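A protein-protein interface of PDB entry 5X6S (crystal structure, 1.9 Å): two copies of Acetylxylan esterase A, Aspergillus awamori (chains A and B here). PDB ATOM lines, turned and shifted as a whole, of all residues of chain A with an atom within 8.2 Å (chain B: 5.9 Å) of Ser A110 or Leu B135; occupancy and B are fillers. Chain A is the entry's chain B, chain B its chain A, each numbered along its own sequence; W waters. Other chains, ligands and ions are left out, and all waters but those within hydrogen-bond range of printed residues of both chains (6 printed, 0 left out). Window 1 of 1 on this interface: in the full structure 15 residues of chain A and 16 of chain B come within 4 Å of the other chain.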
ATOM      1  N   ASN A  30       3.477 -20.902 -22.389  1.00  0.00           N
ATOM      2  CA  ASN A  30       3.809 -19.530 -22.038  1.00  0.00           C
ATOM      3  C   ASN A  30       5.188 -19.277 -22.648  1.00  0.00           C
ATOM      4  O   ASN A  30       6.203 -19.415 -21.947  1.00  0.00           O
ATOM      5  CB  ASN A  30       3.910 -19.437 -20.513  1.00  0.00           C
ATOM      6  CG  ASN A  30       2.564 -19.680 -19.848  1.00  0.00           C
ATOM      7  OD1 ASN A  30       1.699 -18.831 -19.912  1.00  0.00           O
ATOM      8  ND2 ASN A  30       2.408 -20.809 -19.258  1.00  0.00           N
ATOM      9  N   PRO A  31       5.226 -18.986 -23.948  1.00  0.00           N
ATOM     10  CA  PRO A  31       6.498 -18.953 -24.646  1.00  0.00           C
ATOM     11  C   PRO A  31       7.426 -17.820 -24.254  1.00  0.00           C
ATOM     12  O   PRO A  31       6.976 -16.699 -23.974  1.00  0.00           O
ATOM     13  CB  PRO A  31       6.072 -18.809 -26.111  1.00  0.00           C
ATOM     14  CG  PRO A  31       4.758 -18.161 -26.061  1.00  0.00           C
ATOM     15  CD  PRO A  31       4.096 -18.674 -24.846  1.00  0.00           C
ATOM     16  N   GLY A  32       8.725 -18.086 -24.303  1.00  0.00           N
ATOM     17  CA  GLY A  32       9.715 -17.036 -24.277  1.00  0.00           C
ATOM     18  C   GLY A  32       9.773 -16.326 -25.623  1.00  0.00           C
ATOM     19  O   GLY A  32       9.003 -16.646 -26.578  1.00  0.00           O
ATOM     20  N   ILE A  33      10.679 -15.356 -25.704  1.00  0.00           N
ATOM     21  CA  ILE A  33      10.935 -14.604 -26.942  1.00  0.00           C
ATOM     22  C   ILE A  33      12.423 -14.454 -27.135  1.00  0.00           C
ATOM     23  O   ILE A  33      13.115 -14.093 -26.191  1.00  0.00           O
ATOM     24  CB  ILE A  33      10.273 -13.208 -26.895  1.00  0.00           C
ATOM     25  CG1 ILE A  33       8.714 -13.315 -26.968  1.00  0.00           C
ATOM     26  CG2 ILE A  33      10.731 -12.339 -28.108  1.00  0.00           C
ATOM     27  CD1 ILE A  33       8.011 -12.047 -26.619  1.00  0.00           C
ATOM     28  N   VAL A  99       8.531  -6.429 -29.333  1.00  0.00           N
ATOM     29  CA  VAL A  99       8.566  -7.259 -28.149  1.00  0.00           C
ATOM     30  C   VAL A  99       7.202  -7.173 -27.438  1.00  0.00           C
ATOM     31  O   VAL A  99       6.609  -8.203 -27.143  1.00  0.00           O
ATOM     32  CB  VAL A  99       9.743  -6.898 -27.239  1.00  0.00           C
ATOM     33  CG1 VAL A  99       9.601  -7.585 -25.888  1.00  0.00           C
ATOM     34  CG2 VAL A  99      11.061  -7.350 -27.899  1.00  0.00           C
ATOM     35  N   THR A 100       6.741  -5.957 -27.135  1.00  0.00           N
ATOM     36  CA  THR A 100       5.563  -5.846 -26.291  1.00  0.00           C
ATOM     37  C   THR A 100       4.322  -6.296 -27.052  1.00  0.00           C
ATOM     38  O   THR A 100       3.418  -6.871 -26.431  1.00  0.00           O
ATOM     39  CB  THR A 100       5.400  -4.451 -25.725  1.00  0.00           C
ATOM     40  OG1 THR A 100       5.272  -3.527 -26.798  1.00  0.00           O
ATOM     41  CG2 THR A 100       6.633  -4.055 -24.829  1.00  0.00           C
ATOM     42  N   ILE A 103       4.383 -10.137 -26.778  1.00  0.00           N
ATOM     43  CA  ILE A 103       4.083 -10.600 -25.431  1.00  0.00           C
ATOM     44  C   ILE A 103       2.558 -10.679 -25.258  1.00  0.00           C
ATOM     45  O   ILE A 103       2.012 -11.692 -24.793  1.00  0.00           O
ATOM     46  CB  ILE A 103       4.676  -9.671 -24.362  1.00  0.00           C
ATOM     47  CG1 ILE A 103       6.201  -9.923 -24.267  1.00  0.00           C
ATOM     48  CG2 ILE A 103       3.940  -9.877 -23.031  1.00  0.00           C
ATOM     49  CD1 ILE A 103       6.978  -8.851 -23.479  1.00  0.00           C
ATOM     50  N   SER A 104       1.879  -9.615 -25.624  1.00  0.00           N
ATOM     51  CA  SER A 104       0.415  -9.583 -25.521  1.00  0.00           C
ATOM     52  C   SER A 104      -0.310 -10.521 -26.523  1.00  0.00           C
ATOM     53  O   SER A 104      -1.184 -11.310 -26.135  1.00  0.00           O
ATOM     54  CB  SER A 104      -0.119  -8.154 -25.658  1.00  0.00           C
ATOM     55  OG  SER A 104      -1.540  -8.170 -25.508  1.00  0.00           O
ATOM     56  N   GLY A 107       0.635 -14.255 -25.482  1.00  0.00           N
ATOM     57  CA  GLY A 107       0.726 -14.612 -24.056  1.00  0.00           C
ATOM     58  C   GLY A 107       2.110 -15.082 -23.729  1.00  0.00           C
ATOM     59  O   GLY A 107       2.311 -16.004 -22.909  1.00  0.00           O
ATOM     60  N   ALA A 108       3.102 -14.445 -24.365  1.00  0.00           N
ATOM     61  CA  ALA A 108       4.519 -14.813 -24.104  1.00  0.00           C
ATOM     62  C   ALA A 108       4.950 -14.381 -22.694  1.00  0.00           C
ATOM     63  O   ALA A 108       4.362 -13.466 -22.086  1.00  0.00           O
ATOM     64  CB  ALA A 108       5.448 -14.200 -25.178  1.00  0.00           C
ATOM     65  N   ASP A 109       5.913 -15.063 -22.134  1.00  0.00           N
ATOM     66  CA  ASP A 109       6.322 -14.765 -20.797  1.00  0.00           C
ATOM     67  C   ASP A 109       7.290 -13.594 -20.807  1.00  0.00           C
ATOM     68  O   ASP A 109       8.410 -13.738 -21.228  1.00  0.00           O
ATOM     69  CB  ASP A 109       6.942 -15.995 -20.157  1.00  0.00           C
ATOM     70  CG  ASP A 109       7.077 -15.869 -18.670  1.00  0.00           C
ATOM     71  OD1 ASP A 109       7.342 -14.750 -18.166  1.00  0.00           O
ATOM     72  OD2 ASP A 109       6.941 -16.924 -18.005  1.00  0.00           O
ATOM     73  N   SER A 110       6.890 -12.457 -20.238  1.00  0.00           N
ATOM     74  CA  SER A 110       7.754 -11.248 -20.276  1.00  0.00           C
ATOM     75  C   SER A 110       9.104 -11.364 -19.517  1.00  0.00           C
ATOM     76  O   SER A 110      10.041 -10.566 -19.730  1.00  0.00           O
ATOM     77  CB  SER A 110       6.969  -9.994 -19.856  1.00  0.00           C
ATOM     78  OG  SER A 110       7.054  -9.837 -18.466  1.00  0.00           O
ATOM     79  N   SER A 111       9.203 -12.369 -18.641  1.00  0.00           N
ATOM     80  CA  SER A 111      10.404 -12.601 -17.861  1.00  0.00           C
ATOM     81  C   SER A 111      11.376 -13.464 -18.657  1.00  0.00           C
ATOM     82  O   SER A 111      12.472 -13.736 -18.197  1.00  0.00           O
ATOM     83  CB  SER A 111      10.057 -13.344 -16.551  1.00  0.00           C
ATOM     84  OG  SER A 111       9.536 -14.659 -16.787  1.00  0.00           O
ATOM     85  N   LYS A 112      10.944 -13.945 -19.825  1.00  0.00           N
ATOM     86  CA  LYS A 112      11.794 -14.830 -20.659  1.00  0.00           C
ATOM     87  C   LYS A 112      12.025 -14.238 -22.080  1.00  0.00           C
ATOM     88  O   LYS A 112      11.774 -14.905 -23.085  1.00  0.00           O
ATOM     89  CB  LYS A 112      11.182 -16.262 -20.778  1.00  0.00           C
ATOM     90  CG  LYS A 112      11.086 -16.989 -19.413  1.00  0.00           C
ATOM     91  CD  LYS A 112      10.311 -18.289 -19.476  1.00  0.00           C
ATOM     92  CE  LYS A 112      10.241 -18.927 -18.081  1.00  0.00           C
ATOM     93  NZ  LYS A 112       9.734 -20.338 -18.246  1.00  0.00           N
ATOM     94  N   VAL A 113      12.515 -13.002 -22.139  1.00  0.00           N
ATOM     95  CA  VAL A 113      12.734 -12.260 -23.394  1.00  0.00           C
ATOM     96  C   VAL A 113      14.225 -11.949 -23.530  1.00  0.00           C
ATOM     97  O   VAL A 113      14.842 -11.417 -22.584  1.00  0.00           O
ATOM     98  CB  VAL A 113      11.879 -10.992 -23.481  1.00  0.00           C
ATOM     99  CG1 VAL A 113      12.155 -10.189 -24.767  1.00  0.00           C
ATOM    100  CG2 VAL A 113      10.386 -11.340 -23.356  1.00  0.00           C
ATOM    101  N   PHE A 114      14.798 -12.342 -24.665  1.00  0.00           N
ATOM    102  CA  PHE A 114      16.231 -12.282 -24.908  1.00  0.00           C
ATOM    103  C   PHE A 114      16.517 -11.570 -26.226  1.00  0.00           C
ATOM    104  O   PHE A 114      15.651 -11.525 -27.120  1.00  0.00           O
ATOM    105  CB  PHE A 114      16.774 -13.726 -24.910  1.00  0.00           C
ATOM    106  CG  PHE A 114      16.431 -14.457 -23.647  1.00  0.00           C
ATOM    107  CD1 PHE A 114      17.181 -14.250 -22.482  1.00  0.00           C
ATOM    108  CD2 PHE A 114      15.288 -15.238 -23.577  1.00  0.00           C
ATOM    109  CE1 PHE A 114      16.812 -14.865 -21.302  1.00  0.00           C
ATOM    110  CE2 PHE A 114      14.939 -15.865 -22.413  1.00  0.00           C
ATOM    111  CZ  PHE A 114      15.673 -15.659 -21.256  1.00  0.00           C
ATOM    112  N   GLU A 134      14.641  -2.860 -19.360  1.00  0.00           N
ATOM    113  CA  GLU A 134      13.495  -3.448 -18.683  1.00  0.00           C
ATOM    114  C   GLU A 134      12.924  -4.648 -19.423  1.00  0.00           C
ATOM    115  O   GLU A 134      12.214  -5.447 -18.798  1.00  0.00           O
ATOM    116  CB  GLU A 134      12.350  -2.436 -18.435  1.00  0.00           C
ATOM    117  CG  GLU A 134      11.635  -1.905 -19.713  1.00  0.00           C
ATOM    118  CD  GLU A 134      12.404  -0.829 -20.469  1.00  0.00           C
ATOM    119  OE1 GLU A 134      13.584  -0.569 -20.152  1.00  0.00           O
ATOM    120  OE2 GLU A 134      11.831  -0.235 -21.398  1.00  0.00           O
ATOM    121  N   LEU A 135      13.179  -4.743 -20.733  1.00  0.00           N
ATOM    122  CA  LEU A 135      12.564  -5.814 -21.559  1.00  0.00           C
ATOM    123  C   LEU A 135      13.281  -7.149 -21.532  1.00  0.00           C
ATOM    124  O   LEU A 135      12.658  -8.182 -21.819  1.00  0.00           O
ATOM    125  CB  LEU A 135      12.418  -5.379 -23.051  1.00  0.00           C
ATOM    126  CG  LEU A 135      11.483  -4.182 -23.328  1.00  0.00           C
ATOM    127  CD1 LEU A 135      11.326  -3.917 -24.841  1.00  0.00           C
ATOM    128  CD2 LEU A 135      10.154  -4.472 -22.723  1.00  0.00           C
ATOM    129  N   PHE A 136      14.571  -7.147 -21.213  1.00  0.00           N
ATOM    130  CA  PHE A 136      15.456  -8.269 -21.525  1.00  0.00           C
ATOM    131  C   PHE A 136      16.137  -8.929 -20.318  1.00  0.00           C
ATOM    132  O   PHE A 136      16.808  -8.259 -19.553  1.00  0.00           O
ATOM    133  CB  PHE A 136      16.529  -7.816 -22.531  1.00  0.00           C
ATOM    134  CG  PHE A 136      15.968  -7.255 -23.818  1.00  0.00           C
ATOM    135  CD1 PHE A 136      15.342  -8.099 -24.749  1.00  0.00           C
ATOM    136  CD2 PHE A 136      15.987  -5.878 -24.081  1.00  0.00           C
ATOM    137  CE1 PHE A 136      14.773  -7.561 -25.904  1.00  0.00           C
ATOM    138  CE2 PHE A 136      15.438  -5.358 -25.250  1.00  0.00           C
ATOM    139  CZ  PHE A 136      14.839  -6.224 -26.173  1.00  0.00           C
ATOM    140  N   ALA A 137      15.997 -10.257 -20.219  1.00  0.00           N
ATOM    141  CA  ALA A 137      16.636 -11.016 -19.157  1.00  0.00           C
ATOM    142  C   ALA A 137      18.104 -11.239 -19.438  1.00  0.00           C
ATOM    143  O   ALA A 137      18.931 -11.238 -18.532  1.00  0.00           O
ATOM    144  CB  ALA A 137      15.925 -12.355 -18.976  1.00  0.00           C
ATOM    145  N   ILE B  95      -4.883 -10.554 -14.373  1.00  0.00           N
ATOM    146  CA  ILE B  95      -4.417  -9.200 -14.137  1.00  0.00           C
ATOM    147  C   ILE B  95      -3.111  -8.944 -14.900  1.00  0.00           C
ATOM    148  O   ILE B  95      -2.921  -7.876 -15.522  1.00  0.00           O
ATOM    149  CB  ILE B  95      -4.251  -8.914 -12.616  1.00  0.00           C
ATOM    150  CG1 ILE B  95      -5.637  -8.958 -11.924  1.00  0.00           C
ATOM    151  CG2 ILE B  95      -3.601  -7.553 -12.397  1.00  0.00           C
ATOM    152  CD1 ILE B  95      -5.541  -8.803 -10.409  1.00  0.00           C
ATOM    153  N   ALA B  96      -2.218  -9.920 -14.889  1.00  0.00           N
ATOM    154  CA  ALA B  96      -0.970  -9.848 -15.643  1.00  0.00           C
ATOM    155  C   ALA B  96      -1.232  -9.554 -17.129  1.00  0.00           C
ATOM    156  O   ALA B  96      -0.575  -8.674 -17.726  1.00  0.00           O
ATOM    157  CB  ALA B  96      -0.206 -11.122 -15.505  1.00  0.00           C
ATOM    158  N   ASN B  97      -2.178 -10.275 -17.722  1.00  0.00           N
ATOM    159  CA  ASN B  97      -2.549 -10.097 -19.109  1.00  0.00           C
ATOM    160  C   ASN B  97      -3.166  -8.735 -19.428  1.00  0.00           C
ATOM    161  O   ASN B  97      -2.984  -8.171 -20.537  1.00  0.00           O
ATOM    162  CB  ASN B  97      -3.411 -11.281 -19.567  1.00  0.00           C
ATOM    163  CG  ASN B  97      -2.656 -12.587 -19.585  1.00  0.00           C
ATOM    164  OD1 ASN B  97      -1.426 -12.598 -19.629  1.00  0.00           O
ATOM    165  ND2 ASN B  97      -3.376 -13.707 -19.503  1.00  0.00           N
ATOM    166  N   VAL B  99      -2.201  -6.019 -17.969  1.00  0.00           N
ATOM    167  CA  VAL B  99      -1.003  -5.223 -18.048  1.00  0.00           C
ATOM    168  C   VAL B  99      -0.368  -5.278 -19.425  1.00  0.00           C
ATOM    169  O   VAL B  99      -0.102  -4.237 -20.053  1.00  0.00           O
ATOM    170  CB  VAL B  99      -0.013  -5.558 -16.896  1.00  0.00           C
ATOM    171  CG1 VAL B  99       1.385  -4.979 -17.173  1.00  0.00           C
ATOM    172  CG2 VAL B  99      -0.563  -5.043 -15.610  1.00  0.00           C
ATOM    173  N   THR B 100      -0.091  -6.494 -19.904  1.00  0.00           N
ATOM    174  CA  THR B 100       0.662  -6.624 -21.129  1.00  0.00           C
ATOM    175  C   THR B 100      -0.137  -6.117 -22.320  1.00  0.00           C
ATOM    176  O   THR B 100       0.449  -5.525 -23.237  1.00  0.00           O
ATOM    177  CB  THR B 100       1.148  -8.063 -21.350  1.00  0.00           C
ATOM    178  OG1 THR B 100       0.007  -8.917 -21.519  1.00  0.00           O
ATOM    179  CG2 THR B 100       2.069  -8.526 -20.161  1.00  0.00           C
ATOM    180  N   ILE B 103       0.174  -2.307 -22.212  1.00  0.00           N
ATOM    181  CA  ILE B 103       1.523  -1.890 -22.661  1.00  0.00           C
ATOM    182  C   ILE B 103       1.534  -1.795 -24.174  1.00  0.00           C
ATOM    183  O   ILE B 103       1.915  -0.735 -24.765  1.00  0.00           O
ATOM    184  CB  ILE B 103       2.653  -2.806 -22.168  1.00  0.00           C
ATOM    185  CG1 ILE B 103       2.835  -2.635 -20.635  1.00  0.00           C
ATOM    186  CG2 ILE B 103       3.966  -2.451 -22.917  1.00  0.00           C
ATOM    187  CD1 ILE B 103       3.664  -3.729 -19.969  1.00  0.00           C
ATOM    188  N   SER B 110       6.987  -0.049 -20.187  1.00  0.00           N
ATOM    189  CA  SER B 110       6.972  -1.249 -19.356  1.00  0.00           C
ATOM    190  C   SER B 110       7.854  -1.185 -18.121  1.00  0.00           C
ATOM    191  O   SER B 110       7.685  -1.979 -17.228  1.00  0.00           O
ATOM    192  CB  SER B 110       7.225  -2.537 -20.165  1.00  0.00           C
ATOM    193  OG  SER B 110       8.579  -2.813 -20.289  1.00  0.00           O
ATOM    194  N   VAL B 113       5.388   0.447 -14.484  1.00  0.00           N
ATOM    195  CA  VAL B 113       4.136  -0.245 -14.191  1.00  0.00           C
ATOM    196  C   VAL B 113       4.096  -0.550 -12.694  1.00  0.00           C
ATOM    197  O   VAL B 113       5.078  -1.080 -12.117  1.00  0.00           O
ATOM    198  CB  VAL B 113       3.949  -1.532 -15.070  1.00  0.00           C
ATOM    199  CG1 VAL B 113       2.613  -2.212 -14.796  1.00  0.00           C
ATOM    200  CG2 VAL B 113       4.123  -1.235 -16.546  1.00  0.00           C
ATOM    201  N   PHE B 114       2.989  -0.184 -12.055  1.00  0.00           N
ATOM    202  CA  PHE B 114       2.881  -0.190 -10.600  1.00  0.00           C
ATOM    203  C   PHE B 114       1.589  -0.882 -10.229  1.00  0.00           C
ATOM    204  O   PHE B 114       0.674  -0.862 -11.017  1.00  0.00           O
ATOM    205  CB  PHE B 114       2.920   1.272 -10.088  1.00  0.00           C
ATOM    206  CG  PHE B 114       4.150   1.995 -10.548  1.00  0.00           C
ATOM    207  CD1 PHE B 114       5.377   1.794  -9.891  1.00  0.00           C
ATOM    208  CD2 PHE B 114       4.105   2.844 -11.645  1.00  0.00           C
ATOM    209  CE1 PHE B 114       6.549   2.398 -10.371  1.00  0.00           C
ATOM    210  CE2 PHE B 114       5.280   3.473 -12.111  1.00  0.00           C
ATOM    211  CZ  PHE B 114       6.505   3.231 -11.461  1.00  0.00           C
ATOM    212  N   MET B 128       0.398 -10.469  -6.691  1.00  0.00           N
ATOM    213  CA  MET B 128       0.908 -10.019  -8.021  1.00  0.00           C
ATOM    214  C   MET B 128       2.412  -9.797  -7.981  1.00  0.00           C
ATOM    215  O   MET B 128       3.121 -10.112  -8.926  1.00  0.00           O
ATOM    216  CB  MET B 128       0.242  -8.718  -8.467  1.00  0.00           C
ATOM    217  CG  MET B 128      -1.266  -8.832  -8.842  1.00  0.00           C
ATOM    218  SD  MET B 128      -1.614 -10.111 -10.088  1.00  0.00           S
ATOM    219  CE  MET B 128      -0.498  -9.563 -11.400  1.00  0.00           C
ATOM    220  N   TYR B 132       3.919 -12.401 -10.625  1.00  0.00           N
ATOM    221  CA  TYR B 132       4.386 -11.665 -11.831  1.00  0.00           C
ATOM    222  C   TYR B 132       5.395 -10.542 -11.478  1.00  0.00           C
ATOM    223  O   TYR B 132       5.242  -9.401 -11.891  1.00  0.00           O
ATOM    224  CB  TYR B 132       3.174 -11.196 -12.712  1.00  0.00           C
ATOM    225  CG  TYR B 132       2.323 -12.373 -13.020  1.00  0.00           C
ATOM    226  CD1 TYR B 132       2.558 -13.148 -14.160  1.00  0.00           C
ATOM    227  CD2 TYR B 132       1.341 -12.809 -12.118  1.00  0.00           C
ATOM    228  CE1 TYR B 132       1.828 -14.285 -14.401  1.00  0.00           C
ATOM    229  CE2 TYR B 132       0.598 -13.948 -12.359  1.00  0.00           C
ATOM    230  CZ  TYR B 132       0.872 -14.694 -13.503  1.00  0.00           C
ATOM    231  OH  TYR B 132       0.168 -15.849 -13.719  1.00  0.00           O
ATOM    232  N   PRO B 133       6.460 -10.873 -10.682  1.00  0.00           N
ATOM    233  CA  PRO B 133       7.426  -9.822 -10.272  1.00  0.00           C
ATOM    234  C   PRO B 133       8.019  -9.030 -11.441  1.00  0.00           C
ATOM    235  O   PRO B 133       8.275  -7.837 -11.307  1.00  0.00           O
ATOM    236  CB  PRO B 133       8.526 -10.624  -9.557  1.00  0.00           C
ATOM    237  CG  PRO B 133       8.396 -12.026 -10.107  1.00  0.00           C
ATOM    238  CD  PRO B 133       6.908 -12.206 -10.236  1.00  0.00           C
ATOM    239  N   GLU B 134       8.171  -9.692 -12.594  1.00  0.00           N
ATOM    240  CA  GLU B 134       8.723  -9.111 -13.829  1.00  0.00           C
ATOM    241  C   GLU B 134       7.954  -7.924 -14.381  1.00  0.00           C
ATOM    242  O   GLU B 134       8.521  -7.129 -15.089  1.00  0.00           O
ATOM    243  CB  GLU B 134       8.858 -10.181 -14.936  1.00  0.00           C
ATOM    244  CG  GLU B 134       7.537 -10.706 -15.570  1.00  0.00           C
ATOM    245  CD  GLU B 134       6.797 -11.777 -14.775  1.00  0.00           C
ATOM    246  OE1 GLU B 134       7.240 -12.109 -13.648  1.00  0.00           O
ATOM    247  OE2 GLU B 134       5.759 -12.303 -15.263  1.00  0.00           O
ATOM    248  N   LEU B 135       6.654  -7.813 -14.058  1.00  0.00           N
ATOM    249  CA  LEU B 135       5.841  -6.741 -14.610  1.00  0.00           C
ATOM    250  C   LEU B 135       5.931  -5.385 -13.856  1.00  0.00           C
ATOM    251  O   LEU B 135       5.655  -4.332 -14.441  1.00  0.00           O
ATOM    252  CB  LEU B 135       4.372  -7.186 -14.685  1.00  0.00           C
ATOM    253  CG  LEU B 135       4.072  -8.318 -15.646  1.00  0.00           C
ATOM    254  CD1 LEU B 135       2.583  -8.678 -15.557  1.00  0.00           C
ATOM    255  CD2 LEU B 135       4.487  -8.012 -17.083  1.00  0.00           C
ATOM    256  N   PHE B 136       6.335  -5.418 -12.579  1.00  0.00           N
ATOM    257  CA  PHE B 136       6.082  -4.313 -11.654  1.00  0.00           C
ATOM    258  C   PHE B 136       7.362  -3.694 -11.094  1.00  0.00           C
ATOM    259  O   PHE B 136       8.203  -4.411 -10.555  1.00  0.00           O
ATOM    260  CB  PHE B 136       5.178  -4.746 -10.525  1.00  0.00           C
ATOM    261  CG  PHE B 136       3.848  -5.266 -10.990  1.00  0.00           C
ATOM    262  CD1 PHE B 136       2.920  -4.402 -11.574  1.00  0.00           C
ATOM    263  CD2 PHE B 136       3.569  -6.628 -10.919  1.00  0.00           C
ATOM    264  CE1 PHE B 136       1.726  -4.879 -12.061  1.00  0.00           C
ATOM    265  CE2 PHE B 136       2.394  -7.130 -11.414  1.00  0.00           C
ATOM    266  CZ  PHE B 136       1.447  -6.262 -11.981  1.00  0.00           C
ATOM    267  N   ALA B 137       7.480  -2.357 -11.246  1.00  0.00           N
ATOM    268  CA  ALA B 137       8.585  -1.565 -10.729  1.00  0.00           C
ATOM    269  C   ALA B 137       8.451  -1.334  -9.241  1.00  0.00           C
ATOM    270  O   ALA B 137       9.447  -1.283  -8.515  1.00  0.00           O
ATOM    271  CB  ALA B 137       8.636  -0.233 -11.459  1.00  0.00           C
HETATM  272  O   HOH W   1      -2.136  -9.484 -23.065  1.00  0.00           O
HETATM  273  O   HOH W   2       9.315  -0.220 -22.269  1.00  0.00           O
HETATM  274  O   HOH W   3       0.584 -11.508 -21.900  1.00  0.00           O
HETATM  275  O   HOH W   4       4.797  -0.928 -26.137  1.00  0.00           O
HETATM  276  O   HOH W   5       3.170  -6.251 -23.638  1.00  0.00           O
HETATM  277  O   HOH W   6       4.752 -12.032 -17.958  1.00  0.00           O
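Among the printed residues, merely in contact across the chains: Ser A110 with Glu B134 (3.1 Å), Glu A134 with Ser B110 (3.2 Å), Leu A135 with Ser B110 (3.3 Å), Ser A110 with Leu B135 (3.4 Å), Ser A104 with Thr B100 (3.6 Å), Thr A100 with Ile B103 (3.7 Å), Ile A103 with Thr B100 (3.7 Å) and Ser A111 with Glu B134 (3.7 Å).
Thr A100 touches Ile B103, and with the chains exchanged Ile A103 touches Thr B100. Ser A110 touches Glu B134, and with the chains exchanged Glu A134 touches Ser B110. Ser A110 touches Leu B135, and with the chains exchanged Leu A135 touches Ser B110. 10 positions are printed for both chains. Of the 8 pairs that touch across the chains among the printed residues, 6 have their exchanged pair printed and touching as well.
Water W2 lies within hydrogen-bond range of OE2 of Glu A134 and N of Ser B110. Water W3 lies within hydrogen-bond range of OG1 of Thr B100, OD1 of Asn B97 and O of Ile A103. Water W1 lies within hydrogen-bond range of OG1 of Thr B100 (2.7 Å), OG of Ser A104 (2.8 Å) and O of Asn B97 (3.0 Å). Water W4 bridges the side-chain hydroxyl of Thr A100 (2.7 Å) and the backbone carbonyl oxygen of Ile B103 (3.2 Å). Water W5 lies within hydrogen-bond range of O of Thr B100 and O of Thr A100. Water W6 bridges OE2 of Glu B134 (2.9 Å) and N of Ser A110 (3.2 Å).
The side-chain hydroxyl (OG1) of Thr B100 is in hydrogen-bond range of the backbone carbonyl oxygen (O) of Asn B97, 3.2 Å away. N of Ala A108 lies within hydrogen-bond range of O of Ile A103 (3.0 Å). OD1 of Asp A109 is in hydrogen-bond range of OG of Ser A111 (2.6 Å).
Printed residues of chain B that touch a printed residue of chain A: Thr B100, Ile B103, Ser B110, Glu B134 and Leu B135. Among the printed residues, 8 pairs touch across the chains. Among the printed residues, no Asp or Glu carboxylate lies within 4 Å of a Lys or Arg side-chain nitrogen of the other chain.
Val A99 touches none of the printed residues of chain B. Of the printed residues of chain B, Thr A100 touches Ile B103 (3.7 Å). Ser A110 touches just these residues of chain B: Glu B134 and Leu B135. Of the printed residues of chain B, Ser A111 touches Glu B134. Printed residues of chain A within 4 Å of Glu B134: Ser A110 and Ser A111. Leu B135 touches just one residue of chain A: Ser A110. The nearest residue of chain B that does not touch Ser A110 is Thr B100 (5.1 Å).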
